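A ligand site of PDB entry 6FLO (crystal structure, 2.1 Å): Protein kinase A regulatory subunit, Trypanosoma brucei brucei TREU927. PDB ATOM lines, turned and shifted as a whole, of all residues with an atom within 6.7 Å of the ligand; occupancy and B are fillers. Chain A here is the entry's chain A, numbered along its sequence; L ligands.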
ATOM      1  N   MET A  73     -21.790 -13.015   4.816  1.00  0.00           N
ATOM      2  CA  MET A  73     -21.988 -12.466   6.145  1.00  0.00           C
ATOM      3  C   MET A  73     -21.079 -11.250   6.273  1.00  0.00           C
ATOM      4  O   MET A  73     -20.113 -11.113   5.529  1.00  0.00           O
ATOM      5  CB  MET A  73     -21.697 -13.502   7.241  1.00  0.00           C
ATOM      6  CG  MET A  73     -20.325 -14.162   7.151  1.00  0.00           C
ATOM      7  SD  MET A  73     -20.264 -15.799   7.928  1.00  0.00           S
ATOM      8  CE  MET A  73     -21.696 -16.584   7.198  1.00  0.00           C
ATOM      9  N   ALA A  75     -18.903  -8.531   8.909  1.00  0.00           N
ATOM     10  CA  ALA A  75     -18.292  -8.374  10.208  1.00  0.00           C
ATOM     11  C   ALA A  75     -19.174  -7.515  11.107  1.00  0.00           C
ATOM     12  O   ALA A  75     -19.608  -6.428  10.728  1.00  0.00           O
ATOM     13  CB  ALA A  75     -16.899  -7.748  10.056  1.00  0.00           C
ATOM     14  N   LEU A  83     -24.349 -21.923   8.788  1.00  0.00           N
ATOM     15  CA  LEU A  83     -23.075 -22.362   8.260  1.00  0.00           C
ATOM     16  C   LEU A  83     -23.222 -22.501   6.747  1.00  0.00           C
ATOM     17  O   LEU A  83     -24.293 -22.841   6.249  1.00  0.00           O
ATOM     18  CB  LEU A  83     -22.688 -23.694   8.914  1.00  0.00           C
ATOM     19  CG  LEU A  83     -21.391 -24.427   8.583  1.00  0.00           C
ATOM     20  CD1 LEU A  83     -20.191 -23.628   8.972  1.00  0.00           C
ATOM     21  CD2 LEU A  83     -21.368 -25.745   9.312  1.00  0.00           C
ATOM     22  N   ILE A  93     -11.955 -13.562   3.032  1.00  0.00           N
ATOM     23  CA  ILE A  93     -12.167 -13.231   4.433  1.00  0.00           C
ATOM     24  C   ILE A  93     -11.560 -11.851   4.675  1.00  0.00           C
ATOM     25  O   ILE A  93     -10.362 -11.636   4.431  1.00  0.00           O
ATOM     26  CB  ILE A  93     -11.538 -14.296   5.353  1.00  0.00           C
ATOM     27  CG1 ILE A  93     -12.010 -15.710   4.976  1.00  0.00           C
ATOM     28  CG2 ILE A  93     -11.868 -14.019   6.805  1.00  0.00           C
ATOM     29  CD1 ILE A  93     -13.510 -15.871   4.906  1.00  0.00           C
ATOM     30  N   LYS A  95     -10.969  -8.671   7.271  1.00  0.00           N
ATOM     31  CA  LYS A  95     -10.957  -8.115   8.622  1.00  0.00           C
ATOM     32  C   LYS A  95     -10.413  -6.696   8.581  1.00  0.00           C
ATOM     33  O   LYS A  95      -9.308  -6.459   8.058  1.00  0.00           O
ATOM     34  CB  LYS A  95     -10.087  -8.964   9.559  1.00  0.00           C
ATOM     35  CG  LYS A  95     -10.565 -10.402   9.823  1.00  0.00           C
ATOM     36  CD  LYS A  95     -10.102 -10.828  11.214  1.00  0.00           C
ATOM     37  CE  LYS A  95     -10.313 -12.314  11.489  1.00  0.00           C
ATOM     38  NZ  LYS A  95      -9.064 -13.070  11.081  1.00  0.00           N
ATOM     39  N   VAL A 100      -7.609 -11.315   4.470  1.00  0.00           N
ATOM     40  CA  VAL A 100      -6.718 -12.072   5.341  1.00  0.00           C
ATOM     41  C   VAL A 100      -6.772 -13.571   5.089  1.00  0.00           C
ATOM     42  O   VAL A 100      -5.965 -14.310   5.673  1.00  0.00           O
ATOM     43  CB  VAL A 100      -6.997 -11.767   6.826  1.00  0.00           C
ATOM     44  CG1 VAL A 100      -6.952 -10.257   7.074  1.00  0.00           C
ATOM     45  CG2 VAL A 100      -8.346 -12.330   7.212  1.00  0.00           C
ATOM     46  N   TYR A 101      -7.655 -14.041   4.216  1.00  0.00           N
ATOM     47  CA  TYR A 101      -7.786 -15.475   4.001  1.00  0.00           C
ATOM     48  C   TYR A 101      -8.701 -15.694   2.817  1.00  0.00           C
ATOM     49  O   TYR A 101      -9.588 -14.881   2.546  1.00  0.00           O
ATOM     50  CB  TYR A 101      -8.356 -16.175   5.245  1.00  0.00           C
ATOM     51  CG  TYR A 101      -8.093 -17.664   5.282  1.00  0.00           C
ATOM     52  CD1 TYR A 101      -6.909 -18.167   5.804  1.00  0.00           C
ATOM     53  CD2 TYR A 101      -9.036 -18.571   4.800  1.00  0.00           C
ATOM     54  CE1 TYR A 101      -6.653 -19.524   5.845  1.00  0.00           C
ATOM     55  CE2 TYR A 101      -8.789 -19.921   4.828  1.00  0.00           C
ATOM     56  CZ  TYR A 101      -7.593 -20.394   5.349  1.00  0.00           C
ATOM     57  OH  TYR A 101      -7.337 -21.748   5.399  1.00  0.00           O
ATOM     58  N   LEU A 102      -8.484 -16.791   2.116  1.00  0.00           N
ATOM     59  CA  LEU A 102      -9.291 -17.144   0.953  1.00  0.00           C
ATOM     60  C   LEU A 102      -9.951 -18.497   1.192  1.00  0.00           C
ATOM     61  O   LEU A 102      -9.262 -19.484   1.484  1.00  0.00           O
ATOM     62  CB  LEU A 102      -8.425 -17.175  -0.317  1.00  0.00           C
ATOM     63  CG  LEU A 102      -9.115 -17.625  -1.590  1.00  0.00           C
ATOM     64  CD1 LEU A 102     -10.023 -16.524  -2.101  1.00  0.00           C
ATOM     65  CD2 LEU A 102      -8.091 -18.015  -2.656  1.00  0.00           C
ATOM     66  N   LYS A 103     -11.265 -18.534   1.077  1.00  0.00           N
ATOM     67  CA  LYS A 103     -12.058 -19.747   1.218  1.00  0.00           C
ATOM     68  C   LYS A 103     -12.330 -20.308  -0.167  1.00  0.00           C
ATOM     69  O   LYS A 103     -12.918 -19.626  -1.005  1.00  0.00           O
ATOM     70  CB  LYS A 103     -13.372 -19.423   1.940  1.00  0.00           C
ATOM     71  CG  LYS A 103     -13.240 -19.232   3.443  1.00  0.00           C
ATOM     72  CD  LYS A 103     -12.998 -20.560   4.179  1.00  0.00           C
ATOM     73  CE  LYS A 103     -12.751 -20.336   5.661  1.00  0.00           C
ATOM     74  NZ  LYS A 103     -12.897 -21.594   6.439  1.00  0.00           N
ATOM     75  N   ALA A 108     -15.813 -24.279   4.580  1.00  0.00           N
ATOM     76  CA  ALA A 108     -17.006 -23.765   5.243  1.00  0.00           C
ATOM     77  C   ALA A 108     -16.761 -22.348   5.733  1.00  0.00           C
ATOM     78  O   ALA A 108     -15.633 -21.959   6.010  1.00  0.00           O
ATOM     79  CB  ALA A 108     -17.400 -24.660   6.424  1.00  0.00           C
ATOM     80  N   VAL A 109     -17.839 -21.559   5.821  1.00  0.00           N
ATOM     81  CA  VAL A 109     -17.781 -20.249   6.456  1.00  0.00           C
ATOM     82  C   VAL A 109     -18.911 -20.163   7.454  1.00  0.00           C
ATOM     83  O   VAL A 109     -19.996 -20.711   7.250  1.00  0.00           O
ATOM     84  CB  VAL A 109     -17.854 -19.087   5.444  1.00  0.00           C
ATOM     85  CG1 VAL A 109     -16.590 -19.026   4.617  1.00  0.00           C
ATOM     86  CG2 VAL A 109     -19.057 -19.221   4.544  1.00  0.00           C
ATOM     87  N   GLY A 110     -18.652 -19.469   8.564  1.00  0.00           N
ATOM     88  CA  GLY A 110     -19.651 -19.264   9.572  1.00  0.00           C
ATOM     89  C   GLY A 110     -19.489 -20.100  10.815  1.00  0.00           C
ATOM     90  O   GLY A 110     -20.264 -19.913  11.759  1.00  0.00           O
ATOM     91  N   GLU A 111     -18.509 -21.011  10.858  1.00  0.00           N
ATOM     92  CA  GLU A 111     -18.434 -21.995  11.941  1.00  0.00           C
ATOM     93  C   GLU A 111     -18.018 -21.335  13.259  1.00  0.00           C
ATOM     94  O   GLU A 111     -18.493 -21.747  14.330  1.00  0.00           O
ATOM     95  CB  GLU A 111     -17.473 -23.123  11.574  1.00  0.00           C
ATOM     96  CG  GLU A 111     -16.021 -22.759  11.769  1.00  0.00           C
ATOM     97  CD  GLU A 111     -15.451 -21.865  10.666  1.00  0.00           C
ATOM     98  OE1 GLU A 111     -16.175 -21.544   9.686  1.00  0.00           O
ATOM     99  OE2 GLU A 111     -14.256 -21.496  10.769  1.00  0.00           O
ATOM    100  N   LEU A 112     -17.130 -20.337  13.203  1.00  0.00           N
ATOM    101  CA  LEU A 112     -16.680 -19.685  14.427  1.00  0.00           C
ATOM    102  C   LEU A 112     -17.852 -19.102  15.192  1.00  0.00           C
ATOM    103  O   LEU A 112     -17.927 -19.230  16.418  1.00  0.00           O
ATOM    104  CB  LEU A 112     -15.659 -18.598  14.104  1.00  0.00           C
ATOM    105  CG  LEU A 112     -14.275 -18.947  13.563  1.00  0.00           C
ATOM    106  CD1 LEU A 112     -13.380 -17.727  13.583  1.00  0.00           C
ATOM    107  CD2 LEU A 112     -13.637 -20.094  14.355  1.00  0.00           C
ATOM    108  N   GLU A 113     -18.783 -18.458  14.492  1.00  0.00           N
ATOM    109  CA  GLU A 113     -19.930 -17.868  15.169  1.00  0.00           C
ATOM    110  C   GLU A 113     -20.869 -18.942  15.693  1.00  0.00           C
ATOM    111  O   GLU A 113     -21.535 -18.727  16.713  1.00  0.00           O
ATOM    112  CB  GLU A 113     -20.669 -16.915  14.236  1.00  0.00           C
ATOM    113  CG  GLU A 113     -19.823 -15.735  13.767  1.00  0.00           C
ATOM    114  CD  GLU A 113     -18.744 -16.147  12.775  1.00  0.00           C
ATOM    115  OE1 GLU A 113     -18.908 -17.203  12.126  1.00  0.00           O
ATOM    116  OE2 GLU A 113     -17.729 -15.439  12.670  1.00  0.00           O
ATOM    117  N   LEU A 114     -20.978 -20.075  15.000  1.00  0.00           N
ATOM    118  CA  LEU A 114     -21.854 -21.144  15.469  1.00  0.00           C
ATOM    119  C   LEU A 114     -21.267 -21.836  16.706  1.00  0.00           C
ATOM    120  O   LEU A 114     -21.997 -22.139  17.646  1.00  0.00           O
ATOM    121  CB  LEU A 114     -22.111 -22.150  14.361  1.00  0.00           C
ATOM    122  CG  LEU A 114     -22.884 -21.595  13.162  1.00  0.00           C
ATOM    123  CD1 LEU A 114     -23.225 -22.690  12.162  1.00  0.00           C
ATOM    124  CD2 LEU A 114     -24.123 -20.832  13.589  1.00  0.00           C
ATOM    125  N   PRO A 119     -20.781 -12.399  17.648  1.00  0.00           N
ATOM    126  CA  PRO A 119     -21.151 -11.764  16.382  1.00  0.00           C
ATOM    127  C   PRO A 119     -20.168 -12.176  15.303  1.00  0.00           C
ATOM    128  O   PRO A 119     -19.057 -12.629  15.569  1.00  0.00           O
ATOM    129  CB  PRO A 119     -21.049 -10.261  16.687  1.00  0.00           C
ATOM    130  CG  PRO A 119     -21.067 -10.174  18.185  1.00  0.00           C
ATOM    131  CD  PRO A 119     -20.370 -11.406  18.656  1.00  0.00           C
ATOM    132  N   THR A 120     -20.579 -11.985  14.045  1.00  0.00           N
ATOM    133  CA  THR A 120     -19.724 -12.387  12.928  1.00  0.00           C
ATOM    134  C   THR A 120     -18.370 -11.702  13.031  1.00  0.00           C
ATOM    135  O   THR A 120     -18.289 -10.465  13.084  1.00  0.00           O
ATOM    136  CB  THR A 120     -20.391 -12.066  11.596  1.00  0.00           C
ATOM    137  OG1 THR A 120     -21.725 -12.583  11.600  1.00  0.00           O
ATOM    138  CG2 THR A 120     -19.616 -12.697  10.447  1.00  0.00           C
ATOM    139  N   VAL A 121     -17.309 -12.513  13.047  1.00  0.00           N
ATOM    140  CA  VAL A 121     -15.963 -11.993  13.224  1.00  0.00           C
ATOM    141  C   VAL A 121     -15.488 -11.236  11.989  1.00  0.00           C
ATOM    142  O   VAL A 121     -14.978 -10.116  12.084  1.00  0.00           O
ATOM    143  CB  VAL A 121     -15.011 -13.153  13.565  1.00  0.00           C
ATOM    144  CG1 VAL A 121     -13.585 -12.644  13.736  1.00  0.00           C
ATOM    145  CG2 VAL A 121     -15.493 -13.891  14.792  1.00  0.00           C
ATOM    146  N   ALA A 122     -15.654 -11.833  10.823  1.00  0.00           N
ATOM    147  CA  ALA A 122     -15.109 -11.302   9.579  1.00  0.00           C
ATOM    148  C   ALA A 122     -16.209 -11.154   8.542  1.00  0.00           C
ATOM    149  O   ALA A 122     -17.266 -11.780   8.625  1.00  0.00           O
ATOM    150  CB  ALA A 122     -13.976 -12.183   9.035  1.00  0.00           C
ATOM    151  N   THR A 123     -15.950 -10.313   7.550  1.00  0.00           N
ATOM    152  CA  THR A 123     -16.807 -10.222   6.377  1.00  0.00           C
ATOM    153  C   THR A 123     -16.345 -11.235   5.348  1.00  0.00           C
ATOM    154  O   THR A 123     -15.155 -11.429   5.131  1.00  0.00           O
ATOM    155  CB  THR A 123     -16.779  -8.804   5.815  1.00  0.00           C
ATOM    156  OG1 THR A 123     -17.589  -7.970   6.639  1.00  0.00           O
ATOM    157  CG2 THR A 123     -17.317  -8.783   4.384  1.00  0.00           C
ATOM    158  N   VAL A 124     -17.310 -11.914   4.724  1.00  0.00           N
ATOM    159  CA  VAL A 124     -17.051 -12.938   3.718  1.00  0.00           C
ATOM    160  C   VAL A 124     -17.655 -12.477   2.407  1.00  0.00           C
ATOM    161  O   VAL A 124     -18.881 -12.441   2.256  1.00  0.00           O
ATOM    162  CB  VAL A 124     -17.609 -14.303   4.123  1.00  0.00           C
ATOM    163  CG1 VAL A 124     -17.220 -15.358   3.076  1.00  0.00           C
ATOM    164  CG2 VAL A 124     -17.103 -14.692   5.511  1.00  0.00           C
ATOM    165  N   ASP A 170      -1.366 -20.868  10.138  1.00  0.00           N
ATOM    166  CA  ASP A 170      -1.687 -19.736  10.985  1.00  0.00           C
ATOM    167  C   ASP A 170      -2.517 -20.227  12.165  1.00  0.00           C
ATOM    168  O   ASP A 170      -2.737 -21.436  12.345  1.00  0.00           O
ATOM    169  CB  ASP A 170      -2.399 -18.627  10.185  1.00  0.00           C
ATOM    170  CG  ASP A 170      -3.818 -18.981   9.773  1.00  0.00           C
ATOM    171  OD1 ASP A 170      -4.359 -20.014  10.234  1.00  0.00           O
ATOM    172  OD2 ASP A 170      -4.441 -18.179   9.039  1.00  0.00           O
ATOM    173  N   TYR A 172      -5.803 -19.732  13.015  1.00  0.00           N
ATOM    174  CA  TYR A 172      -7.058 -20.307  12.551  1.00  0.00           C
ATOM    175  C   TYR A 172      -6.857 -21.712  11.999  1.00  0.00           C
ATOM    176  O   TYR A 172      -7.712 -22.590  12.182  1.00  0.00           O
ATOM    177  CB  TYR A 172      -7.674 -19.395  11.486  1.00  0.00           C
ATOM    178  CG  TYR A 172      -8.946 -19.902  10.856  1.00  0.00           C
ATOM    179  CD1 TYR A 172     -10.189 -19.651  11.436  1.00  0.00           C
ATOM    180  CD2 TYR A 172      -8.914 -20.652   9.687  1.00  0.00           C
ATOM    181  CE1 TYR A 172     -11.348 -20.119  10.857  1.00  0.00           C
ATOM    182  CE2 TYR A 172     -10.064 -21.124   9.099  1.00  0.00           C
ATOM    183  CZ  TYR A 172     -11.286 -20.858   9.695  1.00  0.00           C
ATOM    184  OH  TYR A 172     -12.436 -21.330   9.108  1.00  0.00           O
ATOM    185  N   GLU A 173      -5.738 -21.946  11.314  1.00  0.00           N
ATOM    186  CA  GLU A 173      -5.551 -23.236  10.664  1.00  0.00           C
ATOM    187  C   GLU A 173      -5.118 -24.314  11.661  1.00  0.00           C
ATOM    188  O   GLU A 173      -5.500 -25.481  11.534  1.00  0.00           O
ATOM    189  CB  GLU A 173      -4.537 -23.116   9.522  1.00  0.00           C
ATOM    190  CG  GLU A 173      -5.075 -22.276   8.378  1.00  0.00           C
ATOM    191  CD  GLU A 173      -4.012 -21.878   7.387  1.00  0.00           C
ATOM    192  OE1 GLU A 173      -2.835 -21.759   7.789  1.00  0.00           O
ATOM    193  OE2 GLU A 173      -4.345 -21.678   6.202  1.00  0.00           O
HETATM  194  N1  LIG L   1     -12.962 -16.671   9.268  1.00  0.00           N
HETATM  195  C1  LIG L   1     -11.670 -16.967   9.038  1.00  0.00           C
HETATM  196  N2  LIG L   1     -11.058 -17.794   8.175  1.00  0.00           N
HETATM  197  C2  LIG L   1      -9.700 -17.889   8.180  1.00  0.00           C
HETATM  198  N3  LIG L   1      -8.983 -17.152   9.055  1.00  0.00           N
HETATM  199  C3  LIG L   1      -9.596 -16.338   9.912  1.00  0.00           C
HETATM  200  O1  LIG L   1      -8.731 -15.651  10.755  1.00  0.00           O
HETATM  201  C4  LIG L   1     -10.974 -16.237   9.915  1.00  0.00           C
HETATM  202  N4  LIG L   1     -11.820 -15.505  10.661  1.00  0.00           N
HETATM  203  C5  LIG L   1     -13.081 -15.775  10.261  1.00  0.00           C
HETATM  204  C6  LIG L   1     -17.062 -15.277   9.557  1.00  0.00           C
HETATM  205  O2  LIG L   1     -16.295 -14.591  10.539  1.00  0.00           O
HETATM  206  C7  LIG L   1     -16.346 -16.521   9.070  1.00  0.00           C
HETATM  207  O3  LIG L   1     -15.093 -16.145   8.443  1.00  0.00           O
HETATM  208  C8  LIG L   1     -14.162 -17.190   8.601  1.00  0.00           C
HETATM  209  C9  LIG L   1     -14.819 -18.296   9.430  1.00  0.00           C
HETATM  210  O4  LIG L   1     -15.354 -19.268   8.529  1.00  0.00           O
HETATM  211  C10 LIG L   1     -15.919 -17.523  10.123  1.00  0.00           C
HETATM  212  O5  LIG L   1     -16.983 -18.339  10.579  1.00  0.00           O
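NZ of Lys 95 sits at hydrogen-bond distance from O1 of the ligand, at 2.6 Å.
The backbone NH (N) of Glu 111 lies within hydrogen-bond range of an oxygen (O5) of the ligand, 3.1 Å away.
The side-chain carboxylate (OE1) of Glu 111 is in hydrogen-bond range of an oxygen (O4) of the ligand, 2.7 Å away.
The side-chain carboxylate (OE2) of Glu 113 lies within hydrogen-bond range of an oxygen (O2) of the ligand.
N of Ala 122 sits at hydrogen-bond distance from O2 of the ligand.
An oxygen (O5) of the ligand is in hydrogen-bond range of the backbone NH of Gly 110, 2.9 Å away.
The backbone NH (N) of Leu 112 sits at hydrogen-bond distance from an oxygen (O5) of the ligand.
N of Val 121 lies within hydrogen-bond range of O2 of the ligand, 3.4 Å away.
Met 73 touches the ligand.
Ile 93 touches the ligand (CG2 to C1, 3.7 Å).
CG of Tyr 101 touches C2 of the ligand (3.3 Å).
Lys 103 touches the ligand (CE to N2, 3.96 Å).
Ala 108 touches the ligand.
Val 109 touches the ligand (CA to O4, 3.3 Å).
Thr 120 touches the ligand (CG2 to C6, 3.7 Å).
CG2 of Val 124 touches O3 of the ligand, at 3.8 Å.
CD2 of Tyr 172 touches C2 of the ligand, at 3.2 Å.
Hydrophobic or aromatic side chains within 4 Å of the ligand: Met 73, Ile 93, Tyr 101, Val 109, Leu 112, Val 121, Ala 122, Val 124 and Tyr 172.
Within 4 Å of the ligand: Met 73, Ile 93, Lys 95, Tyr 101, Lys 103, Ala 108, Val 109, Gly 110, Glu 111, Leu 112, Glu 113, Thr 120, Val 121, Ala 122, Val 124 and Tyr 172.
Along chain A the residues within 4 Å of the ligand span positions 73 to 172.
The nearest printed residue that does not touch the ligand is Asp 170 (4.7 Å).
OE2 of Glu 111 is in hydrogen-bond range of OH of Tyr 172.
The side-chain carboxylate (OE2) of Glu 113 sits at hydrogen-bond distance from the backbone NH (N) of Val 121 (3.0 Å).
OH of Tyr 172 is in hydrogen-bond range of NZ of Lys 103, at 2.7 Å.
The backbone NH (N) of Tyr 172 sits at hydrogen-bond distance from the side-chain carboxylate (OD1) of Asp 170.
The backbone carbonyl oxygen of Tyr 101 sits at hydrogen-bond distance from the backbone NH of Ile 93, 2.8 Å away.
The backbone carbonyl oxygen (O) of Met 73 is in hydrogen-bond range of the backbone NH (N) of Val 124 (3.0 Å).
The side-chain amino group (NZ) of Lys 103 is in hydrogen-bond range of the backbone carbonyl oxygen (O) of Ala 108.
The backbone carbonyl oxygen (O) of Ile 93 is in hydrogen-bond range of the backbone NH (N) of Val 100 (2.8 Å).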
